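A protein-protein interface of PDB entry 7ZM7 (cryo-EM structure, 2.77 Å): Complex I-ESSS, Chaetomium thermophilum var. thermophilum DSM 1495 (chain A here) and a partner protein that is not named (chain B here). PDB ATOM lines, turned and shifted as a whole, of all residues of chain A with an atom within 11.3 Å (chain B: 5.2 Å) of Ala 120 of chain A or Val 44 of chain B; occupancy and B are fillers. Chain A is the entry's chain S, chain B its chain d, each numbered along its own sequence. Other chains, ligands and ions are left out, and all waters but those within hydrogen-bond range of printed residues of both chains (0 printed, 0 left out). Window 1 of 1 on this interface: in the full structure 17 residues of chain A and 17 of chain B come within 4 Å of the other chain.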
ATOM      1  N   ASP A 113       4.704 -40.480 -28.546  1.00  0.00           N
ATOM      2  CA  ASP A 113       5.900 -39.845 -28.006  1.00  0.00           C
ATOM      3  C   ASP A 113       5.596 -39.301 -26.622  1.00  0.00           C
ATOM      4  O   ASP A 113       4.866 -38.322 -26.482  1.00  0.00           O
ATOM      5  CB  ASP A 113       6.392 -38.729 -28.916  1.00  0.00           C
ATOM      6  CG  ASP A 113       7.707 -38.156 -28.453  1.00  0.00           C
ATOM      7  OD1 ASP A 113       8.743 -38.832 -28.645  1.00  0.00           O
ATOM      8  OD2 ASP A 113       7.707 -37.049 -27.881  1.00  0.00           O
ATOM      9  N   THR A 114       6.160 -39.935 -25.600  1.00  0.00           N
ATOM     10  CA  THR A 114       6.047 -39.466 -24.226  1.00  0.00           C
ATOM     11  C   THR A 114       7.345 -38.850 -23.732  1.00  0.00           C
ATOM     12  O   THR A 114       7.639 -38.901 -22.539  1.00  0.00           O
ATOM     13  CB  THR A 114       5.613 -40.599 -23.299  1.00  0.00           C
ATOM     14  OG1 THR A 114       6.571 -41.658 -23.347  1.00  0.00           O
ATOM     15  CG2 THR A 114       4.274 -41.148 -23.735  1.00  0.00           C
ATOM     16  N   SER A 115       8.133 -38.282 -24.634  1.00  0.00           N
ATOM     17  CA  SER A 115       9.337 -37.576 -24.241  1.00  0.00           C
ATOM     18  C   SER A 115       8.989 -36.286 -23.503  1.00  0.00           C
ATOM     19  O   SER A 115       7.966 -35.657 -23.759  1.00  0.00           O
ATOM     20  CB  SER A 115      10.184 -37.264 -25.468  1.00  0.00           C
ATOM     21  OG  SER A 115      11.422 -36.703 -25.078  1.00  0.00           O
ATOM     22  N   ILE A 116       9.812 -35.928 -22.513  1.00  0.00           N
ATOM     23  CA  ILE A 116       9.563 -34.702 -21.694  1.00  0.00           C
ATOM     24  C   ILE A 116       9.719 -33.472 -22.583  1.00  0.00           C
ATOM     25  O   ILE A 116       9.143 -32.427 -22.261  1.00  0.00           O
ATOM     26  CB  ILE A 116      10.516 -34.625 -20.479  1.00  0.00           C
ATOM     27  CG1 ILE A 116      10.214 -33.440 -19.561  1.00  0.00           C
ATOM     28  CG2 ILE A 116      11.968 -34.624 -20.930  1.00  0.00           C
ATOM     29  CD1 ILE A 116       8.821 -33.433 -18.991  1.00  0.00           C
ATOM     30  N   GLN A 117      10.404 -33.614 -23.709  1.00  0.00           N
ATOM     31  CA  GLN A 117      10.704 -32.407 -24.508  1.00  0.00           C
ATOM     32  C   GLN A 117       9.481 -32.054 -25.344  1.00  0.00           C
ATOM     33  O   GLN A 117       9.053 -30.904 -25.285  1.00  0.00           O
ATOM     34  CB  GLN A 117      11.918 -32.655 -25.400  1.00  0.00           C
ATOM     35  CG  GLN A 117      13.246 -32.419 -24.702  1.00  0.00           C
ATOM     36  CD  GLN A 117      13.926 -33.701 -24.298  1.00  0.00           C
ATOM     37  OE1 GLN A 117      13.311 -34.763 -24.261  1.00  0.00           O
ATOM     38  NE2 GLN A 117      15.209 -33.602 -23.991  1.00  0.00           N
ATOM     39  N   THR A 118       8.891 -33.030 -26.018  1.00  0.00           N
ATOM     40  CA  THR A 118       7.688 -32.726 -26.779  1.00  0.00           C
ATOM     41  C   THR A 118       6.656 -32.033 -25.917  1.00  0.00           C
ATOM     42  O   THR A 118       5.924 -31.168 -26.402  1.00  0.00           O
ATOM     43  CB  THR A 118       7.099 -33.994 -27.383  1.00  0.00           C
ATOM     44  OG1 THR A 118       8.139 -34.743 -28.019  1.00  0.00           O
ATOM     45  CG2 THR A 118       6.038 -33.652 -28.403  1.00  0.00           C
ATOM     46  N   TRP A 119       6.591 -32.391 -24.637  1.00  0.00           N
ATOM     47  CA  TRP A 119       5.700 -31.705 -23.714  1.00  0.00           C
ATOM     48  C   TRP A 119       6.224 -30.327 -23.338  1.00  0.00           C
ATOM     49  O   TRP A 119       5.467 -29.353 -23.330  1.00  0.00           O
ATOM     50  CB  TRP A 119       5.473 -32.571 -22.482  1.00  0.00           C
ATOM     51  CG  TRP A 119       4.456 -31.972 -21.569  1.00  0.00           C
ATOM     52  CD1 TRP A 119       3.162 -32.320 -21.469  1.00  0.00           C
ATOM     53  CD2 TRP A 119       4.682 -30.957 -20.581  1.00  0.00           C
ATOM     54  NE1 TRP A 119       2.547 -31.564 -20.517  1.00  0.00           N
ATOM     55  CE2 TRP A 119       3.463 -30.718 -19.956  1.00  0.00           C
ATOM     56  CE3 TRP A 119       5.800 -30.229 -20.173  1.00  0.00           C
ATOM     57  CZ2 TRP A 119       3.315 -29.775 -18.952  1.00  0.00           C
ATOM     58  CZ3 TRP A 119       5.657 -29.286 -19.198  1.00  0.00           C
ATOM     59  CH2 TRP A 119       4.423 -29.066 -18.591  1.00  0.00           C
ATOM     60  N   ALA A 120       7.508 -30.223 -23.018  1.00  0.00           N
ATOM     61  CA  ALA A 120       8.044 -28.949 -22.567  1.00  0.00           C
ATOM     62  C   ALA A 120       8.111 -27.933 -23.693  1.00  0.00           C
ATOM     63  O   ALA A 120       8.073 -26.732 -23.433  1.00  0.00           O
ATOM     64  CB  ALA A 120       9.429 -29.142 -21.947  1.00  0.00           C
ATOM     65  N   LEU A 121       8.250 -28.389 -24.939  1.00  0.00           N
ATOM     66  CA  LEU A 121       8.238 -27.465 -26.064  1.00  0.00           C
ATOM     67  C   LEU A 121       6.878 -26.820 -26.252  1.00  0.00           C
ATOM     68  O   LEU A 121       6.791 -25.623 -26.535  1.00  0.00           O
ATOM     69  CB  LEU A 121       8.651 -28.164 -27.355  1.00  0.00           C
ATOM     70  CG  LEU A 121      10.100 -28.394 -27.789  1.00  0.00           C
ATOM     71  CD1 LEU A 121      10.742 -27.089 -28.004  1.00  0.00           C
ATOM     72  CD2 LEU A 121      10.921 -29.212 -26.869  1.00  0.00           C
ATOM     73  N   GLU A 122       5.805 -27.593 -26.133  1.00  0.00           N
ATOM     74  CA  GLU A 122       4.490 -27.037 -26.417  1.00  0.00           C
ATOM     75  C   GLU A 122       4.121 -25.946 -25.427  1.00  0.00           C
ATOM     76  O   GLU A 122       3.564 -24.914 -25.816  1.00  0.00           O
ATOM     77  CB  GLU A 122       3.439 -28.133 -26.415  1.00  0.00           C
ATOM     78  CG  GLU A 122       2.065 -27.593 -26.660  1.00  0.00           C
ATOM     79  CD  GLU A 122       0.996 -28.601 -26.414  1.00  0.00           C
ATOM     80  OE1 GLU A 122       1.226 -29.782 -26.743  1.00  0.00           O
ATOM     81  OE2 GLU A 122      -0.069 -28.213 -25.887  1.00  0.00           O
ATOM     82  N   GLU A 123       4.420 -26.156 -24.146  1.00  0.00           N
ATOM     83  CA  GLU A 123       4.201 -25.111 -23.157  1.00  0.00           C
ATOM     84  C   GLU A 123       5.152 -23.947 -23.369  1.00  0.00           C
ATOM     85  O   GLU A 123       4.718 -22.795 -23.494  1.00  0.00           O
ATOM     86  CB  GLU A 123       4.361 -25.677 -21.747  1.00  0.00           C
ATOM     87  CG  GLU A 123       4.206 -24.647 -20.644  1.00  0.00           C
ATOM     88  CD  GLU A 123       2.862 -23.910 -20.678  1.00  0.00           C
ATOM     89  OE1 GLU A 123       1.806 -24.568 -20.661  1.00  0.00           O
ATOM     90  OE2 GLU A 123       2.868 -22.664 -20.732  1.00  0.00           O
ATOM     91  N   ALA A 124       6.455 -24.226 -23.421  1.00  0.00           N
ATOM     92  CA  ALA A 124       7.442 -23.164 -23.582  1.00  0.00           C
ATOM     93  C   ALA A 124       7.190 -22.365 -24.841  1.00  0.00           C
ATOM     94  O   ALA A 124       7.515 -21.178 -24.900  1.00  0.00           O
ATOM     95  CB  ALA A 124       8.848 -23.751 -23.621  1.00  0.00           C
ATOM     96  N   ARG A 125       6.554 -22.956 -25.846  1.00  0.00           N
ATOM     97  CA  ARG A 125       6.204 -22.102 -27.005  1.00  0.00           C
ATOM     98  C   ARG A 125       5.125 -21.151 -26.521  1.00  0.00           C
ATOM     99  O   ARG A 125       5.269 -19.964 -26.775  1.00  0.00           O
ATOM    100  CB  ARG A 125       5.648 -22.887 -28.193  1.00  0.00           C
ATOM    101  CG  ARG A 125       5.850 -22.206 -29.536  1.00  0.00           C
ATOM    102  CD  ARG A 125       5.386 -23.095 -30.672  1.00  0.00           C
ATOM    103  NE  ARG A 125       5.777 -22.578 -31.972  1.00  0.00           N
ATOM    104  CZ  ARG A 125       6.897 -22.908 -32.605  1.00  0.00           C
ATOM    105  NH1 ARG A 125       7.166 -22.384 -33.788  1.00  0.00           N
ATOM    106  NH2 ARG A 125       7.742 -23.761 -32.055  1.00  0.00           N
ATOM    107  N   ARG A 126       4.148 -21.650 -25.757  1.00  0.00           N
ATOM    108  CA  ARG A 126       3.025 -20.789 -25.408  1.00  0.00           C
ATOM    109  C   ARG A 126       3.422 -19.652 -24.486  1.00  0.00           C
ATOM    110  O   ARG A 126       2.782 -18.599 -24.495  1.00  0.00           O
ATOM    111  CB  ARG A 126       1.917 -21.604 -24.764  1.00  0.00           C
ATOM    112  CG  ARG A 126       1.119 -22.407 -25.734  1.00  0.00           C
ATOM    113  CD  ARG A 126      -0.120 -22.893 -25.034  1.00  0.00           C
ATOM    114  NE  ARG A 126       0.202 -23.748 -23.908  1.00  0.00           N
ATOM    115  CZ  ARG A 126       0.337 -25.055 -24.007  1.00  0.00           C
ATOM    116  NH1 ARG A 126       0.637 -25.771 -22.946  1.00  0.00           N
ATOM    117  NH2 ARG A 126       0.129 -25.643 -25.161  1.00  0.00           N
ATOM    118  N   ARG A 127       4.465 -19.858 -23.687  1.00  0.00           N
ATOM    119  CA  ARG A 127       4.957 -18.783 -22.790  1.00  0.00           C
ATOM    120  C   ARG A 127       5.666 -17.725 -23.633  1.00  0.00           C
ATOM    121  O   ARG A 127       5.408 -16.537 -23.412  1.00  0.00           O
ATOM    122  CB  ARG A 127       5.845 -19.376 -21.692  1.00  0.00           C
ATOM    123  CG  ARG A 127       5.098 -20.272 -20.720  1.00  0.00           C
ATOM    124  CD  ARG A 127       5.932 -20.627 -19.510  1.00  0.00           C
ATOM    125  NE  ARG A 127       5.243 -21.615 -18.695  1.00  0.00           N
ATOM    126  CZ  ARG A 127       5.740 -22.153 -17.591  1.00  0.00           C
ATOM    127  NH1 ARG A 127       6.940 -21.798 -17.166  1.00  0.00           N
ATOM    128  NH2 ARG A 127       5.037 -23.046 -16.920  1.00  0.00           N
ATOM    129  N   LEU A 128       6.514 -18.148 -24.570  1.00  0.00           N
ATOM    130  CA  LEU A 128       7.215 -17.199 -25.479  1.00  0.00           C
ATOM    131  C   LEU A 128       6.207 -16.472 -26.374  1.00  0.00           C
ATOM    132  O   LEU A 128       6.487 -15.329 -26.739  1.00  0.00           O
ATOM    133  CB  LEU A 128       8.274 -17.939 -26.296  1.00  0.00           C
ATOM    134  CG  LEU A 128       9.503 -18.387 -25.512  1.00  0.00           C
ATOM    135  CD1 LEU A 128      10.463 -19.142 -26.411  1.00  0.00           C
ATOM    136  CD2 LEU A 128      10.198 -17.200 -24.869  1.00  0.00           C
ATOM    137  N   GLU A 129       5.125 -17.143 -26.767  1.00  0.00           N
ATOM    138  CA  GLU A 129       4.092 -16.540 -27.657  1.00  0.00           C
ATOM    139  C   GLU A 129       3.441 -15.336 -26.970  1.00  0.00           C
ATOM    140  O   GLU A 129       3.095 -14.377 -27.680  1.00  0.00           O
ATOM    141  CB  GLU A 129       3.082 -17.586 -28.119  1.00  0.00           C
ATOM    142  CG  GLU A 129       3.640 -18.482 -29.209  1.00  0.00           C
ATOM    143  CD  GLU A 129       2.609 -19.303 -29.959  1.00  0.00           C
ATOM    144  OE1 GLU A 129       1.407 -19.146 -29.673  1.00  0.00           O
ATOM    145  OE2 GLU A 129       3.015 -20.095 -30.832  1.00  0.00           O
ATOM    146  N   GLU A 131       4.972 -13.296 -25.084  1.00  0.00           N
ATOM    147  CA  GLU A 131       5.982 -12.235 -25.322  1.00  0.00           C
ATOM    148  C   GLU A 131       6.149 -12.040 -26.834  1.00  0.00           C
ATOM    149  O   GLU A 131       5.580 -12.832 -27.602  1.00  0.00           O
ATOM    150  CB  GLU A 131       7.304 -12.636 -24.670  1.00  0.00           C
ATOM    151  CG  GLU A 131       7.129 -13.589 -23.503  1.00  0.00           C
ATOM    152  CD  GLU A 131       8.394 -14.312 -23.074  1.00  0.00           C
ATOM    153  OE1 GLU A 131       9.486 -13.895 -23.502  1.00  0.00           O
ATOM    154  OE2 GLU A 131       8.281 -15.296 -22.319  1.00  0.00           O
ATOM    155  N   ILE A 133       8.729 -12.538 -28.377  1.00  0.00           N
ATOM    156  CA  ILE A 133       9.831 -13.443 -28.809  1.00  0.00           C
ATOM    157  C   ILE A 133       9.346 -14.405 -29.899  1.00  0.00           C
ATOM    158  O   ILE A 133      10.068 -14.564 -30.901  1.00  0.00           O
ATOM    159  CB  ILE A 133      10.354 -14.201 -27.578  1.00  0.00           C
ATOM    160  CG1 ILE A 133      10.849 -13.239 -26.496  1.00  0.00           C
ATOM    161  CG2 ILE A 133      11.437 -15.180 -27.991  1.00  0.00           C
ATOM    162  CD1 ILE A 133      12.012 -12.376 -26.928  1.00  0.00           C
ATOM    163  N   LEU A 134       8.165 -14.999 -29.726  1.00  0.00           N
ATOM    164  CA  LEU A 134       7.611 -15.895 -30.771  1.00  0.00           C
ATOM    165  C   LEU A 134       6.271 -15.325 -31.234  1.00  0.00           C
ATOM    166  O   LEU A 134       5.578 -14.706 -30.405  1.00  0.00           O
ATOM    167  CB  LEU A 134       7.457 -17.310 -30.202  1.00  0.00           C
ATOM    168  CG  LEU A 134       8.516 -18.314 -30.650  1.00  0.00           C
ATOM    169  CD1 LEU A 134       9.856 -18.040 -29.987  1.00  0.00           C
ATOM    170  CD2 LEU A 134       8.069 -19.732 -30.354  1.00  0.00           C
ATOM    171  N   ARG B  40       8.998 -30.323 -14.377  1.00  0.00           N
ATOM    172  CA  ARG B  40       8.461 -29.821 -15.634  1.00  0.00           C
ATOM    173  C   ARG B  40       8.651 -28.313 -15.782  1.00  0.00           C
ATOM    174  O   ARG B  40       8.904 -27.829 -16.888  1.00  0.00           O
ATOM    175  CB  ARG B  40       7.000 -30.224 -15.769  1.00  0.00           C
ATOM    176  CG  ARG B  40       6.849 -31.741 -15.871  1.00  0.00           C
ATOM    177  CD  ARG B  40       5.582 -32.206 -16.542  1.00  0.00           C
ATOM    178  NE  ARG B  40       5.420 -33.640 -16.370  1.00  0.00           N
ATOM    179  CZ  ARG B  40       5.469 -34.538 -17.343  1.00  0.00           C
ATOM    180  NH1 ARG B  40       5.648 -34.171 -18.599  1.00  0.00           N
ATOM    181  NH2 ARG B  40       5.306 -35.813 -17.052  1.00  0.00           N
ATOM    182  N   GLU B  41       8.614 -27.568 -14.683  1.00  0.00           N
ATOM    183  CA  GLU B  41       8.898 -26.120 -14.790  1.00  0.00           C
ATOM    184  C   GLU B  41      10.331 -25.932 -15.271  1.00  0.00           C
ATOM    185  O   GLU B  41      10.515 -25.171 -16.230  1.00  0.00           O
ATOM    186  CB  GLU B  41       8.679 -25.411 -13.459  1.00  0.00           C
ATOM    187  CG  GLU B  41       7.218 -25.152 -13.145  1.00  0.00           C
ATOM    188  CD  GLU B  41       6.548 -24.051 -13.949  1.00  0.00           C
ATOM    189  OE1 GLU B  41       7.254 -23.332 -14.679  1.00  0.00           O
ATOM    190  OE2 GLU B  41       5.317 -23.912 -13.836  1.00  0.00           O
ATOM    191  N   GLN B  42      11.295 -26.640 -14.670  1.00  0.00           N
ATOM    192  CA  GLN B  42      12.722 -26.489 -15.043  1.00  0.00           C
ATOM    193  C   GLN B  42      12.894 -26.848 -16.516  1.00  0.00           C
ATOM    194  O   GLN B  42      13.608 -26.128 -17.210  1.00  0.00           O
ATOM    195  CB  GLN B  42      13.583 -27.416 -14.195  1.00  0.00           C
ATOM    196  CG  GLN B  42      13.591 -27.079 -12.715  1.00  0.00           C
ATOM    197  CD  GLN B  42      14.362 -28.121 -11.945  1.00  0.00           C
ATOM    198  OE1 GLN B  42      14.771 -29.142 -12.488  1.00  0.00           O
ATOM    199  NE2 GLN B  42      14.574 -27.862 -10.667  1.00  0.00           N
ATOM    200  N   TRP B  43      12.182 -27.872 -16.988  1.00  0.00           N
ATOM    201  CA  TRP B  43      12.300 -28.334 -18.396  1.00  0.00           C
ATOM    202  C   TRP B  43      11.668 -27.337 -19.375  1.00  0.00           C
ATOM    203  O   TRP B  43      12.235 -27.161 -20.463  1.00  0.00           O
ATOM    204  CB  TRP B  43      11.691 -29.729 -18.526  1.00  0.00           C
ATOM    205  CG  TRP B  43      12.675 -30.836 -18.313  1.00  0.00           C
ATOM    206  CD1 TRP B  43      12.773 -31.655 -17.228  1.00  0.00           C
ATOM    207  CD2 TRP B  43      13.715 -31.245 -19.218  1.00  0.00           C
ATOM    208  NE1 TRP B  43      13.796 -32.546 -17.396  1.00  0.00           N
ATOM    209  CE2 TRP B  43      14.394 -32.318 -18.605  1.00  0.00           C
ATOM    210  CE3 TRP B  43      14.136 -30.813 -20.478  1.00  0.00           C
ATOM    211  CZ2 TRP B  43      15.468 -32.961 -19.213  1.00  0.00           C
ATOM    212  CZ3 TRP B  43      15.198 -31.451 -21.078  1.00  0.00           C
ATOM    213  CH2 TRP B  43      15.853 -32.511 -20.454  1.00  0.00           C
ATOM    214  N   VAL B  44      10.533 -26.732 -19.025  1.00  0.00           N
ATOM    215  CA  VAL B  44       9.896 -25.694 -19.892  1.00  0.00           C
ATOM    216  C   VAL B  44      10.825 -24.484 -20.001  1.00  0.00           C
ATOM    217  O   VAL B  44      10.900 -23.880 -21.072  1.00  0.00           O
ATOM    218  CB  VAL B  44       8.494 -25.320 -19.376  1.00  0.00           C
ATOM    219  CG1 VAL B  44       8.026 -23.964 -19.871  1.00  0.00           C
ATOM    220  CG2 VAL B  44       7.476 -26.394 -19.695  1.00  0.00           C
ATOM    221  N   GLN B  45      11.492 -24.147 -18.909  1.00  0.00           N
ATOM    222  CA  GLN B  45      12.423 -23.004 -18.896  1.00  0.00           C
ATOM    223  C   GLN B  45      13.596 -23.275 -19.841  1.00  0.00           C
ATOM    224  O   GLN B  45      14.080 -22.319 -20.459  1.00  0.00           O
ATOM    225  CB  GLN B  45      12.793 -22.694 -17.449  1.00  0.00           C
ATOM    226  CG  GLN B  45      11.704 -21.943 -16.707  1.00  0.00           C
ATOM    227  CD  GLN B  45      11.583 -20.531 -17.217  1.00  0.00           C
ATOM    228  OE1 GLN B  45      10.547 -20.123 -17.731  1.00  0.00           O
ATOM    229  NE2 GLN B  45      12.660 -19.775 -17.088  1.00  0.00           N
ATOM    230  N   VAL B  46      14.062 -24.518 -19.916  1.00  0.00           N
ATOM    231  CA  VAL B  46      15.259 -24.782 -20.757  1.00  0.00           C
ATOM    232  C   VAL B  46      14.806 -24.946 -22.204  1.00  0.00           C
ATOM    233  O   VAL B  46      15.584 -24.589 -23.112  1.00  0.00           O
ATOM    234  CB  VAL B  46      16.099 -25.961 -20.237  1.00  0.00           C
ATOM    235  CG1 VAL B  46      17.175 -26.375 -21.227  1.00  0.00           C
ATOM    236  CG2 VAL B  46      16.709 -25.662 -18.877  1.00  0.00           C
ATOM    237  N   MET B  47      13.572 -25.400 -22.413  1.00  0.00           N
ATOM    238  CA  MET B  47      13.085 -25.435 -23.779  1.00  0.00           C
ATOM    239  C   MET B  47      12.686 -24.064 -24.293  1.00  0.00           C
ATOM    240  O   MET B  47      12.685 -23.864 -25.507  1.00  0.00           O
ATOM    241  CB  MET B  47      11.915 -26.402 -23.927  1.00  0.00           C
ATOM    242  CG  MET B  47      12.262 -27.861 -23.684  1.00  0.00           C
ATOM    243  SD  MET B  47      13.481 -28.596 -24.769  1.00  0.00           S
ATOM    244  CE  MET B  47      14.934 -28.600 -23.717  1.00  0.00           C
ATOM    245  N   MET B  48      12.471 -23.111 -23.382  1.00  0.00           N
ATOM    246  CA  MET B  48      12.199 -21.709 -23.796  1.00  0.00           C
ATOM    247  C   MET B  48      13.489 -21.146 -24.392  1.00  0.00           C
ATOM    248  O   MET B  48      13.394 -20.426 -25.395  1.00  0.00           O
ATOM    249  CB  MET B  48      11.753 -20.852 -22.608  1.00  0.00           C
ATOM    250  CG  MET B  48      10.257 -20.736 -22.476  1.00  0.00           C
ATOM    251  SD  MET B  48       9.781 -19.970 -20.918  1.00  0.00           S
ATOM    252  CE  MET B  48      10.381 -18.302 -21.179  1.00  0.00           C
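NH1 of Arg 127 of chain A lies within salt-bridge range of OE1 of Glu 41 of chain B (2.9 Å).
OG of Ser 115 of chain A sits at hydrogen-bond distance from OE1 of Gln 117 of chain A (2.8 Å). The backbone carbonyl oxygen (O) of Leu 128 of chain A lies within hydrogen-bond range of the backbone NH (N) of Leu 134 of chain A, at 3.4 Å. The side-chain carboxylate (OE1) of Glu 123 of chain A is in salt-bridge range of the guanidinium group (NH1) of Arg 126 of chain A (2.8 Å). The side-chain amide oxygen (OE1) of Gln 45 of chain B sits close to the side-chain sulfur (SD) of Met 48 of chain B. NE of Arg 127 of chain A is in salt-bridge range of OE2 of Glu 123 of chain A.
Ile 116 of chain A touches Arg 40 of chain B. CG1 of Ile 116 of chain A touches CG of Trp 43 of chain B (3.8 Å). NE2 of Gln 117 of chain A touches CZ3 of Trp 43 of chain B, at 3.6 Å. CZ3 of Trp 119 of chain A touches CB of Arg 40 of chain B, at 3.8 Å. CB of Ala 120 of chain A touches O of Trp 43 of chain B, 3.7 Å away. CG2 of Val 44 of chain B touches O of Ala 120 of chain A, 3.8 Å away. SD of Met 47 of chain B touches CD2 of Leu 121 of chain A (3.4 Å). Ala 124 of chain A touches Val 44 of chain B. CD1 of Leu 128 of chain A touches O of Met 48 of chain B, 3.4 Å away. Glu 131 of chain A touches Met 48 of chain B.
Printed residues of chain B within 4 Å of Ile 116 of chain A: Arg 40 and Trp 43. Of the printed residues of chain B, Ala 120 of chain A touches Trp 43, Val 44 and Met 47. Of the printed residues of chain B, Arg 127 of chain A touches Glu 41 and Val 44. Printed residues of chain B within 4 Å of Glu 131 of chain A: Met 48 (3.8 Å). Printed residues of chain A within 4 Å of Arg 40 of chain B: Ile 116 (3.3 Å) and Trp 119 (3.8 Å). Glu 41 of chain B touches just one residue of chain A: Arg 127. Of the printed residues of chain A, Trp 43 of chain B touches Ile 116, Gln 117 and Ala 120. No residue of chain A comes within 4 Å of Val 46 of chain B. Of chain A, only Gln 117, Ala 120, Leu 121 and Ala 124 come within 4 Å of Met 47 of chain B. Met 48 of chain B touches three residues of chain A. The nearest printed residue of chain A that does not touch Trp 43 of chain B is Ala 124 of chain A (5.8 Å).
Of the 20 printed residues of chain A, 10 touch a printed residue of chain B. Hydrophobic or aromatic side chains of chain A within 4 Å of the printed part of chain B: Ile 116, Trp 119, Ala 120, Leu 121, Ala 124 and Leu 128. Of the 9 printed residues of chain B, 6 touch a printed residue of chain A. Along chain B the printed residues that touch a printed residue of chain A span positions 40 to 48. Among the printed residues, 18 pairs touch across the chains. Among the printed residues, Asp or Glu carboxylates within 4 Å of a Lys or Arg side-chain nitrogen of the other chain: Arg 127 of chain A with Glu 41 of chain B (2.9 Å).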
